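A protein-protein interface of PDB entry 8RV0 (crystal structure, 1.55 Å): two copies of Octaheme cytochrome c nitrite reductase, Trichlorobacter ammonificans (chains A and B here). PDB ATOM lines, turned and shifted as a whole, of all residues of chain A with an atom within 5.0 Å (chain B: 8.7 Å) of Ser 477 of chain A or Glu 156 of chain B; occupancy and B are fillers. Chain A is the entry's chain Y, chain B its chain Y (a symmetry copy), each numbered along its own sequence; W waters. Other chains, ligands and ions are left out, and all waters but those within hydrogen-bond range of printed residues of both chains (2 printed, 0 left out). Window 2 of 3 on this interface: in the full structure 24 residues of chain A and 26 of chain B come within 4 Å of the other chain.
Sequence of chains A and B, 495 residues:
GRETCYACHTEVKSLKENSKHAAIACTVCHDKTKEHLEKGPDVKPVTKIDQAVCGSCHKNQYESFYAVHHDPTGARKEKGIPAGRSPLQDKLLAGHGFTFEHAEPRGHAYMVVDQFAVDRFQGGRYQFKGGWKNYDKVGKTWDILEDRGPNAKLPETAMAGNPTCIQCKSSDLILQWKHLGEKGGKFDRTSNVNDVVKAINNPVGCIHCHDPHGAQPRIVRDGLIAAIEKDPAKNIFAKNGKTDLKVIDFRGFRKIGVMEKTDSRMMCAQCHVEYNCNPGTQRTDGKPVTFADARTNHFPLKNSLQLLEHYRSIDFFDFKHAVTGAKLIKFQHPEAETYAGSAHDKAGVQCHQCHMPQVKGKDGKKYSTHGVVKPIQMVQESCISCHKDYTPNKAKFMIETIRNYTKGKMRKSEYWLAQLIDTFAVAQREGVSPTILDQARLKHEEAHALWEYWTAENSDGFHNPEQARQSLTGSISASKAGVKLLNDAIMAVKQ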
ATOM      1  N   LYS A 409      26.025 -13.374 -17.048  1.00  0.00           N
ATOM      2  CA  LYS A 409      27.178 -12.494 -16.800  1.00  0.00           C
ATOM      3  C   LYS A 409      28.251 -12.794 -17.840  1.00  0.00           C
ATOM      4  O   LYS A 409      28.961 -11.883 -18.255  1.00  0.00           O
ATOM      5  CB  LYS A 409      27.702 -12.743 -15.381  1.00  0.00           C
ATOM      6  CG  LYS A 409      26.678 -12.421 -14.320  1.00  0.00           C
ATOM      7  CD  LYS A 409      25.993 -11.058 -14.506  1.00  0.00           C
ATOM      8  CE  LYS A 409      25.032 -10.884 -13.355  1.00  0.00           C
ATOM      9  NZ  LYS A 409      24.266  -9.619 -13.359  1.00  0.00           N
ATOM     10  N   ARG A 469      30.848 -15.160 -10.440  1.00  0.00           N
ATOM     11  CA  ARG A 469      30.175 -13.870 -10.416  1.00  0.00           C
ATOM     12  C   ARG A 469      31.284 -12.811 -10.178  1.00  0.00           C
ATOM     13  O   ARG A 469      31.315 -11.769 -10.859  1.00  0.00           O
ATOM     14  CB  ARG A 469      29.058 -13.741  -9.339  1.00  0.00           C
ATOM     15  CG  ARG A 469      28.200 -12.469  -9.502  1.00  0.00           C
ATOM     16  CD  ARG A 469      27.467 -12.011  -8.208  1.00  0.00           C
ATOM     17  NE  ARG A 469      26.698 -10.915  -8.742  1.00  0.00           N
ATOM     18  CZ  ARG A 469      27.123  -9.649  -8.874  1.00  0.00           C
ATOM     19  NH1 ARG A 469      28.330  -9.303  -8.434  1.00  0.00           N
ATOM     20  NH2 ARG A 469      26.313  -8.783  -9.499  1.00  0.00           N
ATOM     21  N   THR A 473      31.985 -10.128 -13.183  1.00  0.00           N
ATOM     22  CA  THR A 473      31.620  -8.730 -12.977  1.00  0.00           C
ATOM     23  C   THR A 473      32.891  -7.881 -13.011  1.00  0.00           C
ATOM     24  O   THR A 473      32.828  -6.682 -13.428  1.00  0.00           O
ATOM     25  CB  THR A 473      30.789  -8.546 -11.700  1.00  0.00           C
ATOM     26  OG1 THR A 473      31.506  -8.965 -10.536  1.00  0.00           O
ATOM     27  CG2 THR A 473      29.470  -9.297 -11.870  1.00  0.00           C
ATOM     28  N   GLY A 474      34.015  -8.483 -12.546  1.00  0.00           N
ATOM     29  CA  GLY A 474      35.323  -7.840 -12.675  1.00  0.00           C
ATOM     30  C   GLY A 474      35.648  -7.584 -14.156  1.00  0.00           C
ATOM     31  O   GLY A 474      36.239  -6.561 -14.529  1.00  0.00           O
ATOM     32  N   SER A 475      35.362  -8.560 -15.018  1.00  0.00           N
ATOM     33  CA  SER A 475      35.624  -8.371 -16.424  1.00  0.00           C
ATOM     34  C   SER A 475      34.834  -7.200 -17.000  1.00  0.00           C
ATOM     35  O   SER A 475      35.341  -6.284 -17.678  1.00  0.00           O
ATOM     36  CB  SER A 475      35.259  -9.693 -17.130  1.00  0.00           C
ATOM     37  OG  SER A 475      35.425  -9.547 -18.517  1.00  0.00           O
ATOM     38  N   ILE A 476      33.520  -7.242 -16.770  1.00  0.00           N
ATOM     39  CA  ILE A 476      32.636  -6.159 -17.184  1.00  0.00           C
ATOM     40  C   ILE A 476      33.221  -4.823 -16.693  1.00  0.00           C
ATOM     41  O   ILE A 476      33.162  -3.860 -17.473  1.00  0.00           O
ATOM     42  CB  ILE A 476      31.213  -6.373 -16.650  1.00  0.00           C
ATOM     43  CG1 ILE A 476      30.669  -7.645 -17.293  1.00  0.00           C
ATOM     44  CG2 ILE A 476      30.312  -5.172 -16.948  1.00  0.00           C
ATOM     45  CD1 ILE A 476      29.373  -8.291 -16.622  1.00  0.00           C
ATOM     46  N   SER A 477      33.639  -4.770 -15.417  1.00  0.00           N
ATOM     47  CA  SER A 477      34.031  -3.448 -14.868  1.00  0.00           C
ATOM     48  C   SER A 477      35.256  -2.940 -15.613  1.00  0.00           C
ATOM     49  O   SER A 477      35.350  -1.720 -15.997  1.00  0.00           O
ATOM     50  CB  SER A 477      34.277  -3.518 -13.380  1.00  0.00           C
ATOM     51  OG  SER A 477      33.106  -3.965 -12.696  1.00  0.00           O
ATOM     52  N   ALA A 478      36.159  -3.910 -15.819  1.00  0.00           N
ATOM     53  CA  ALA A 478      37.389  -3.660 -16.583  1.00  0.00           C
ATOM     54  C   ALA A 478      37.083  -3.153 -17.957  1.00  0.00           C
ATOM     55  O   ALA A 478      37.694  -2.169 -18.364  1.00  0.00           O
ATOM     56  CB  ALA A 478      38.411  -4.775 -16.685  1.00  0.00           C
ATOM     57  N   SER A 479      36.148  -3.807 -18.665  1.00  0.00           N
ATOM     58  CA  SER A 479      35.872  -3.374 -20.028  1.00  0.00           C
ATOM     59  C   SER A 479      35.153  -2.025 -20.099  1.00  0.00           C
ATOM     60  O   SER A 479      35.425  -1.231 -20.990  1.00  0.00           O
ATOM     61  CB  SER A 479      34.953  -4.333 -20.718  1.00  0.00           C
ATOM     62  OG  SER A 479      35.673  -5.512 -20.972  1.00  0.00           O
ATOM     63  N   LYS A 480      34.176  -1.798 -19.217  1.00  0.00           N
ATOM     64  CA  LYS A 480      33.472  -0.510 -19.305  1.00  0.00           C
ATOM     65  C   LYS A 480      34.439   0.650 -18.942  1.00  0.00           C
ATOM     66  O   LYS A 480      34.371   1.737 -19.517  1.00  0.00           O
ATOM     67  CB  LYS A 480      32.417  -0.455 -18.188  1.00  0.00           C
ATOM     68  CG  LYS A 480      31.108  -1.240 -18.374  1.00  0.00           C
ATOM     69  CD  LYS A 480      30.258  -1.284 -17.088  1.00  0.00           C
ATOM     70  CE  LYS A 480      28.858  -1.840 -17.377  1.00  0.00           C
ATOM     71  NZ  LYS A 480      27.875  -1.703 -16.255  1.00  0.00           N
ATOM     72  N   ALA A 481      35.375   0.398 -18.047  1.00  0.00           N
ATOM     73  CA  ALA A 481      36.435   1.371 -17.740  1.00  0.00           C
ATOM     74  C   ALA A 481      37.337   1.689 -18.947  1.00  0.00           C
ATOM     75  O   ALA A 481      37.696   2.862 -19.137  1.00  0.00           O
ATOM     76  CB  ALA A 481      37.211   0.954 -16.528  1.00  0.00           C
ATOM     77  N   ASP B  90      21.735  -5.328 -23.888  1.00  0.00           N
ATOM     78  CA  ASP B  90      22.794  -4.510 -23.340  1.00  0.00           C
ATOM     79  C   ASP B  90      23.025  -3.309 -24.284  1.00  0.00           C
ATOM     80  O   ASP B  90      23.305  -2.239 -23.782  1.00  0.00           O
ATOM     81  CB  ASP B  90      24.083  -5.324 -23.185  1.00  0.00           C
ATOM     82  CG  ASP B  90      24.031  -6.186 -21.920  1.00  0.00           C
ATOM     83  OD1 ASP B  90      24.001  -5.668 -20.760  1.00  0.00           O
ATOM     84  OD2 ASP B  90      23.985  -7.393 -22.097  1.00  0.00           O
ATOM     85  N   GLY B  97      19.155   0.907 -15.819  1.00  0.00           N
ATOM     86  CA  GLY B  97      19.520  -0.068 -14.799  1.00  0.00           C
ATOM     87  C   GLY B  97      19.164  -1.516 -15.209  1.00  0.00           C
ATOM     88  O   GLY B  97      19.669  -2.443 -14.620  1.00  0.00           O
ATOM     89  N   THR B  99      20.257  -3.090 -17.604  1.00  0.00           N
ATOM     90  CA  THR B  99      21.440  -3.716 -18.163  1.00  0.00           C
ATOM     91  C   THR B  99      22.228  -4.429 -17.052  1.00  0.00           C
ATOM     92  O   THR B  99      23.059  -5.245 -17.392  1.00  0.00           O
ATOM     93  CB  THR B  99      22.315  -2.732 -18.968  1.00  0.00           C
ATOM     94  OG1 THR B  99      22.795  -1.792 -18.014  1.00  0.00           O
ATOM     95  CG2 THR B  99      21.652  -2.057 -20.167  1.00  0.00           C
ATOM     96  N   PHE B 100      21.907  -4.201 -15.772  1.00  0.00           N
ATOM     97  CA  PHE B 100      22.647  -4.851 -14.697  1.00  0.00           C
ATOM     98  C   PHE B 100      22.135  -6.283 -14.426  1.00  0.00           C
ATOM     99  O   PHE B 100      22.922  -7.195 -14.139  1.00  0.00           O
ATOM    100  CB  PHE B 100      22.654  -4.019 -13.414  1.00  0.00           C
ATOM    101  CG  PHE B 100      23.602  -2.860 -13.576  1.00  0.00           C
ATOM    102  CD1 PHE B 100      24.967  -3.033 -13.351  1.00  0.00           C
ATOM    103  CD2 PHE B 100      23.090  -1.631 -13.981  1.00  0.00           C
ATOM    104  CE1 PHE B 100      25.836  -1.953 -13.537  1.00  0.00           C
ATOM    105  CE2 PHE B 100      23.940  -0.551 -14.134  1.00  0.00           C
ATOM    106  CZ  PHE B 100      25.297  -0.723 -13.891  1.00  0.00           C
ATOM    107  N   GLU B 101      20.851  -6.497 -14.652  1.00  0.00           N
ATOM    108  CA  GLU B 101      20.212  -7.825 -14.579  1.00  0.00           C
ATOM    109  C   GLU B 101      18.724  -7.678 -14.862  1.00  0.00           C
ATOM    110  O   GLU B 101      18.041  -6.852 -14.257  1.00  0.00           O
ATOM    111  CB  GLU B 101      20.314  -8.531 -13.218  1.00  0.00           C
ATOM    112  CG  GLU B 101      19.643  -9.885 -13.262  1.00  0.00           C
ATOM    113  CD  GLU B 101      19.896 -10.818 -12.070  1.00  0.00           C
ATOM    114  OE1 GLU B 101      20.322 -10.297 -10.973  1.00  0.00           O
ATOM    115  OE2 GLU B 101      19.656 -12.087 -12.182  1.00  0.00           O
ATOM    116  N   VAL B 118      17.330  -9.156  -6.905  1.00  0.00           N
ATOM    117  CA  VAL B 118      17.848  -8.970  -8.264  1.00  0.00           C
ATOM    118  C   VAL B 118      19.004  -7.952  -8.191  1.00  0.00           C
ATOM    119  O   VAL B 118      18.971  -7.035  -7.368  1.00  0.00           O
ATOM    120  CB  VAL B 118      16.724  -8.532  -9.253  1.00  0.00           C
ATOM    121  CG1 VAL B 118      16.307  -7.092  -8.923  1.00  0.00           C
ATOM    122  CG2 VAL B 118      17.167  -8.584 -10.726  1.00  0.00           C
ATOM    123  N   ASP B 119      19.965  -8.090  -9.121  1.00  0.00           N
ATOM    124  CA  ASP B 119      21.205  -7.275  -9.090  1.00  0.00           C
ATOM    125  C   ASP B 119      20.898  -5.788  -9.246  1.00  0.00           C
ATOM    126  O   ASP B 119      21.756  -5.011  -8.895  1.00  0.00           O
ATOM    127  CB  ASP B 119      22.293  -7.706 -10.059  1.00  0.00           C
ATOM    128  CG  ASP B 119      22.915  -9.063  -9.728  1.00  0.00           C
ATOM    129  OD1 ASP B 119      22.692  -9.560  -8.662  1.00  0.00           O
ATOM    130  OD2 ASP B 119      23.688  -9.556 -10.579  1.00  0.00           O
ATOM    131  N   ARG B 120      19.745  -5.417  -9.810  1.00  0.00           N
ATOM    132  CA  ARG B 120      19.440  -4.003 -10.043  1.00  0.00           C
ATOM    133  C   ARG B 120      18.729  -3.354  -8.874  1.00  0.00           C
ATOM    134  O   ARG B 120      18.408  -2.160  -8.994  1.00  0.00           O
ATOM    135  CB  ARG B 120      18.642  -3.825 -11.349  1.00  0.00           C
ATOM    136  CG  ARG B 120      17.235  -4.423 -11.388  1.00  0.00           C
ATOM    137  CD  ARG B 120      16.625  -4.162 -12.788  1.00  0.00           C
ATOM    138  NE  ARG B 120      15.217  -4.436 -12.719  1.00  0.00           N
ATOM    139  CZ  ARG B 120      14.647  -5.641 -12.991  1.00  0.00           C
ATOM    140  NH1 ARG B 120      15.409  -6.668 -13.362  1.00  0.00           N
ATOM    141  NH2 ARG B 120      13.325  -5.851 -12.795  1.00  0.00           N
ATOM    142  N   PHE B 121      18.384  -4.097  -7.807  1.00  0.00           N
ATOM    143  CA  PHE B 121      17.486  -3.564  -6.766  1.00  0.00           C
ATOM    144  C   PHE B 121      18.157  -2.602  -5.756  1.00  0.00           C
ATOM    145  O   PHE B 121      17.756  -1.431  -5.566  1.00  0.00           O
ATOM    146  CB  PHE B 121      16.763  -4.728  -6.081  1.00  0.00           C
ATOM    147  CG  PHE B 121      15.783  -4.250  -5.047  1.00  0.00           C
ATOM    148  CD1 PHE B 121      14.625  -3.551  -5.391  1.00  0.00           C
ATOM    149  CD2 PHE B 121      16.056  -4.466  -3.706  1.00  0.00           C
ATOM    150  CE1 PHE B 121      13.745  -3.159  -4.380  1.00  0.00           C
ATOM    151  CE2 PHE B 121      15.199  -4.025  -2.710  1.00  0.00           C
ATOM    152  CZ  PHE B 121      14.028  -3.407  -3.053  1.00  0.00           C
ATOM    153  N   GLY B 123      21.969  -2.839  -4.835  1.00  0.00           N
ATOM    154  CA  GLY B 123      23.401  -2.989  -4.799  1.00  0.00           C
ATOM    155  C   GLY B 123      23.834  -4.371  -4.297  1.00  0.00           C
ATOM    156  O   GLY B 123      24.912  -4.561  -3.769  1.00  0.00           O
ATOM    157  N   GLY B 124      22.938  -5.349  -4.397  1.00  0.00           N
ATOM    158  CA  GLY B 124      23.285  -6.696  -3.956  1.00  0.00           C
ATOM    159  C   GLY B 124      23.085  -6.862  -2.458  1.00  0.00           C
ATOM    160  O   GLY B 124      23.495  -7.872  -1.921  1.00  0.00           O
ATOM    161  N   LYS B 153      28.946  -3.951  -0.487  1.00  0.00           N
ATOM    162  CA  LYS B 153      28.796  -3.597  -1.886  1.00  0.00           C
ATOM    163  C   LYS B 153      29.010  -4.868  -2.708  1.00  0.00           C
ATOM    164  O   LYS B 153      29.622  -5.842  -2.247  1.00  0.00           O
ATOM    165  CB  LYS B 153      29.640  -2.379  -2.277  1.00  0.00           C
ATOM    166  CG  LYS B 153      30.954  -2.171  -1.519  1.00  0.00           C
ATOM    167  CD  LYS B 153      31.790  -0.993  -2.060  1.00  0.00           C
ATOM    168  CE  LYS B 153      33.031  -0.656  -1.249  1.00  0.00           C
ATOM    169  NZ  LYS B 153      33.110   0.789  -0.894  1.00  0.00           N
ATOM    170  N   LEU B 154      28.284  -4.957  -3.809  1.00  0.00           N
ATOM    171  CA  LEU B 154      28.543  -6.063  -4.701  1.00  0.00           C
ATOM    172  C   LEU B 154      28.758  -5.439  -6.081  1.00  0.00           C
ATOM    173  O   LEU B 154      27.934  -4.656  -6.511  1.00  0.00           O
ATOM    174  CB  LEU B 154      27.281  -6.919  -4.686  1.00  0.00           C
ATOM    175  CG  LEU B 154      27.416  -8.406  -4.432  1.00  0.00           C
ATOM    176  CD1 LEU B 154      26.135  -9.096  -4.876  1.00  0.00           C
ATOM    177  CD2 LEU B 154      28.609  -8.966  -5.167  1.00  0.00           C
ATOM    178  N   PRO B 155      29.821  -5.838  -6.826  1.00  0.00           N
ATOM    179  CA  PRO B 155      30.136  -5.286  -8.136  1.00  0.00           C
ATOM    180  C   PRO B 155      29.036  -5.480  -9.189  1.00  0.00           C
ATOM    181  O   PRO B 155      28.271  -6.443  -9.117  1.00  0.00           O
ATOM    182  CB  PRO B 155      31.460  -5.912  -8.568  1.00  0.00           C
ATOM    183  CG  PRO B 155      31.927  -6.661  -7.363  1.00  0.00           C
ATOM    184  CD  PRO B 155      30.766  -6.893  -6.388  1.00  0.00           C
ATOM    185  N   GLU B 156      28.891  -4.472 -10.052  1.00  0.00           N
ATOM    186  CA  GLU B 156      27.987  -4.525 -11.188  1.00  0.00           C
ATOM    187  C   GLU B 156      26.552  -4.785 -10.701  1.00  0.00           C
ATOM    188  O   GLU B 156      25.871  -5.708 -11.148  1.00  0.00           O
ATOM    189  CB  GLU B 156      28.506  -5.544 -12.221  1.00  0.00           C
ATOM    190  CG  GLU B 156      29.809  -5.110 -12.835  1.00  0.00           C
ATOM    191  CD  GLU B 156      29.679  -3.841 -13.658  1.00  0.00           C
ATOM    192  OE1 GLU B 156      28.590  -3.576 -14.241  1.00  0.00           O
ATOM    193  OE2 GLU B 156      30.703  -3.124 -13.779  1.00  0.00           O
ATOM    194  N   THR B 157      26.123  -3.933  -9.771  1.00  0.00           N
ATOM    195  CA  THR B 157      24.735  -3.854  -9.305  1.00  0.00           C
ATOM    196  C   THR B 157      24.210  -2.461  -9.599  1.00  0.00           C
ATOM    197  O   THR B 157      24.971  -1.569  -9.991  1.00  0.00           O
ATOM    198  CB  THR B 157      24.605  -4.233  -7.827  1.00  0.00           C
ATOM    199  OG1 THR B 157      25.522  -3.399  -7.100  1.00  0.00           O
ATOM    200  CG2 THR B 157      24.950  -5.678  -7.555  1.00  0.00           C
ATOM    201  N   ALA B 158      22.931  -2.256  -9.299  1.00  0.00           N
ATOM    202  CA  ALA B 158      22.276  -0.963  -9.359  1.00  0.00           C
ATOM    203  C   ALA B 158      21.366  -0.777  -8.150  1.00  0.00           C
ATOM    204  O   ALA B 158      21.143  -1.728  -7.396  1.00  0.00           O
ATOM    205  CB  ALA B 158      21.457  -0.765 -10.635  1.00  0.00           C
ATOM    206  N   MET B 159      20.790   0.426  -8.046  1.00  0.00           N
ATOM    207  CA  MET B 159      20.009   0.817  -6.850  1.00  0.00           C
ATOM    208  C   MET B 159      18.675   1.420  -7.302  1.00  0.00           C
ATOM    209  O   MET B 159      18.300   2.546  -6.915  1.00  0.00           O
ATOM    210  CB  MET B 159      20.777   1.887  -6.054  1.00  0.00           C
ATOM    211  CG  MET B 159      22.163   1.408  -5.580  1.00  0.00           C
ATOM    212  SD  MET B 159      21.965   0.550  -4.010  1.00  0.00           S
ATOM    213  CE  MET B 159      21.798   1.945  -2.864  1.00  0.00           C
HETATM  214  O   HOH W   1      25.721  -3.024 -17.330  1.00  0.00           O
HETATM  215  O   HOH W   2      25.494  -7.108 -13.711  1.00  0.00           O
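The side-chain amino group (NZ) of Lys 409 of chain A lies within hydrogen-bond range of the backbone carbonyl oxygen (O) of Phe 100 of chain B.
The side-chain amino group of Lys 409 of chain A is in salt-bridge range of the side-chain carboxylate of Asp 119 of chain B.
NH2 of Arg 469 of chain A lies within salt-bridge range of OD2 of Asp 119 of chain B (2.9 Å).
The backbone carbonyl oxygen of Pro 155 of chain B is in hydrogen-bond range of the guanidinium group of Arg 469 of chain A (2.9 Å).
OE2 of Glu 156 of chain B sits at hydrogen-bond distance from OG of Ser 477 of chain A, 2.8 Å away.
The side-chain amino group of Lys 480 of chain A is in salt-bridge range of the side-chain carboxylate of Glu 156 of chain B.
The backbone carbonyl oxygen (O) of Arg 469 of chain A is in hydrogen-bond range of the side-chain hydroxyl (OG1) of Thr 473 of chain A (2.8 Å).
The side-chain hydroxyl (OG) of Ser 477 of chain A is in hydrogen-bond range of the backbone carbonyl oxygen (O) of Thr 473 of chain A (2.8 Å).
OE1 of Glu 101 of chain B lies within hydrogen-bond range of N of Asp 119 of chain B (2.9 Å).
The backbone NH (N) of Ala 158 of chain B is in hydrogen-bond range of the backbone carbonyl oxygen (O) of Asp 119 of chain B, at 3.0 Å.
O of Gly 123 of chain B lies within hydrogen-bond range of N of Leu 154 of chain B.
OG1 of Thr 157 of chain B lies within hydrogen-bond range of O of Leu 154 of chain B (2.8 Å).
Leu 154 of chain B touches Arg 469 of chain A.
Arg 469 of chain A touches Glu 156 of chain B (NH2 to O, 3.5 Å).
Arg 469 of chain A touches Thr 157 of chain B (NH2 to CG2, 3.9 Å).
CB of Pro 155 of chain B touches OG1 of Thr 473 of chain A (3.6 Å).
Thr 473 of chain A touches Glu 156 of chain B.
Ile 476 of chain A touches Glu 156 of chain B.
Phe 100 of chain B touches Lys 480 of chain A.
Ser 477 of chain A touches just one residue of chain B: Glu 156.
Glu 156 of chain B touches just these residues of chain A: Arg 469, Thr 473, Ile 476, Ser 477 and Lys 480.
No residue of chain B comes within 4 Å of Gly 474 of chain A.
Of the printed residues of chain A, Phe 100 of chain B touches Lys 409 and Lys 480.
Of the printed residues of chain B, Lys 409 of chain A touches Phe 100 and Asp 119.
Of the printed residues of chain A, Leu 154 of chain B touches Arg 469 (3.3 Å).
Of the printed residues of chain B, Thr 473 of chain A touches Pro 155 and Glu 156.
Of the printed residues of chain B, Arg 469 of chain A touches Asp 119, Leu 154, Pro 155, Glu 156 and Thr 157.
Ser 479 of chain A touches none of the printed residues of chain B.
The nearest printed residue of chain A that does not touch Leu 154 of chain B is Thr 473 of chain A (6.1 Å).
Of the 11 printed residues of chain A, 6 touch a printed residue of chain B.
Hydrophobic or aromatic side chains of chain A that line the printed part of chain B: Ile 476.
Among the printed residues, 13 pairs touch across the chains.
No position is printed for both chains.
Water W2 lies within hydrogen-bond range of the backbone carbonyl oxygen of Phe 100 of chain B, the side-chain amino group of Lys 409 of chain A and the backbone carbonyl oxygen of Glu 156 of chain B.
Water W1 lies within hydrogen-bond range of the side-chain amino group of Lys 480 of chain A and the side-chain hydroxyl of Thr 99 of chain B.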
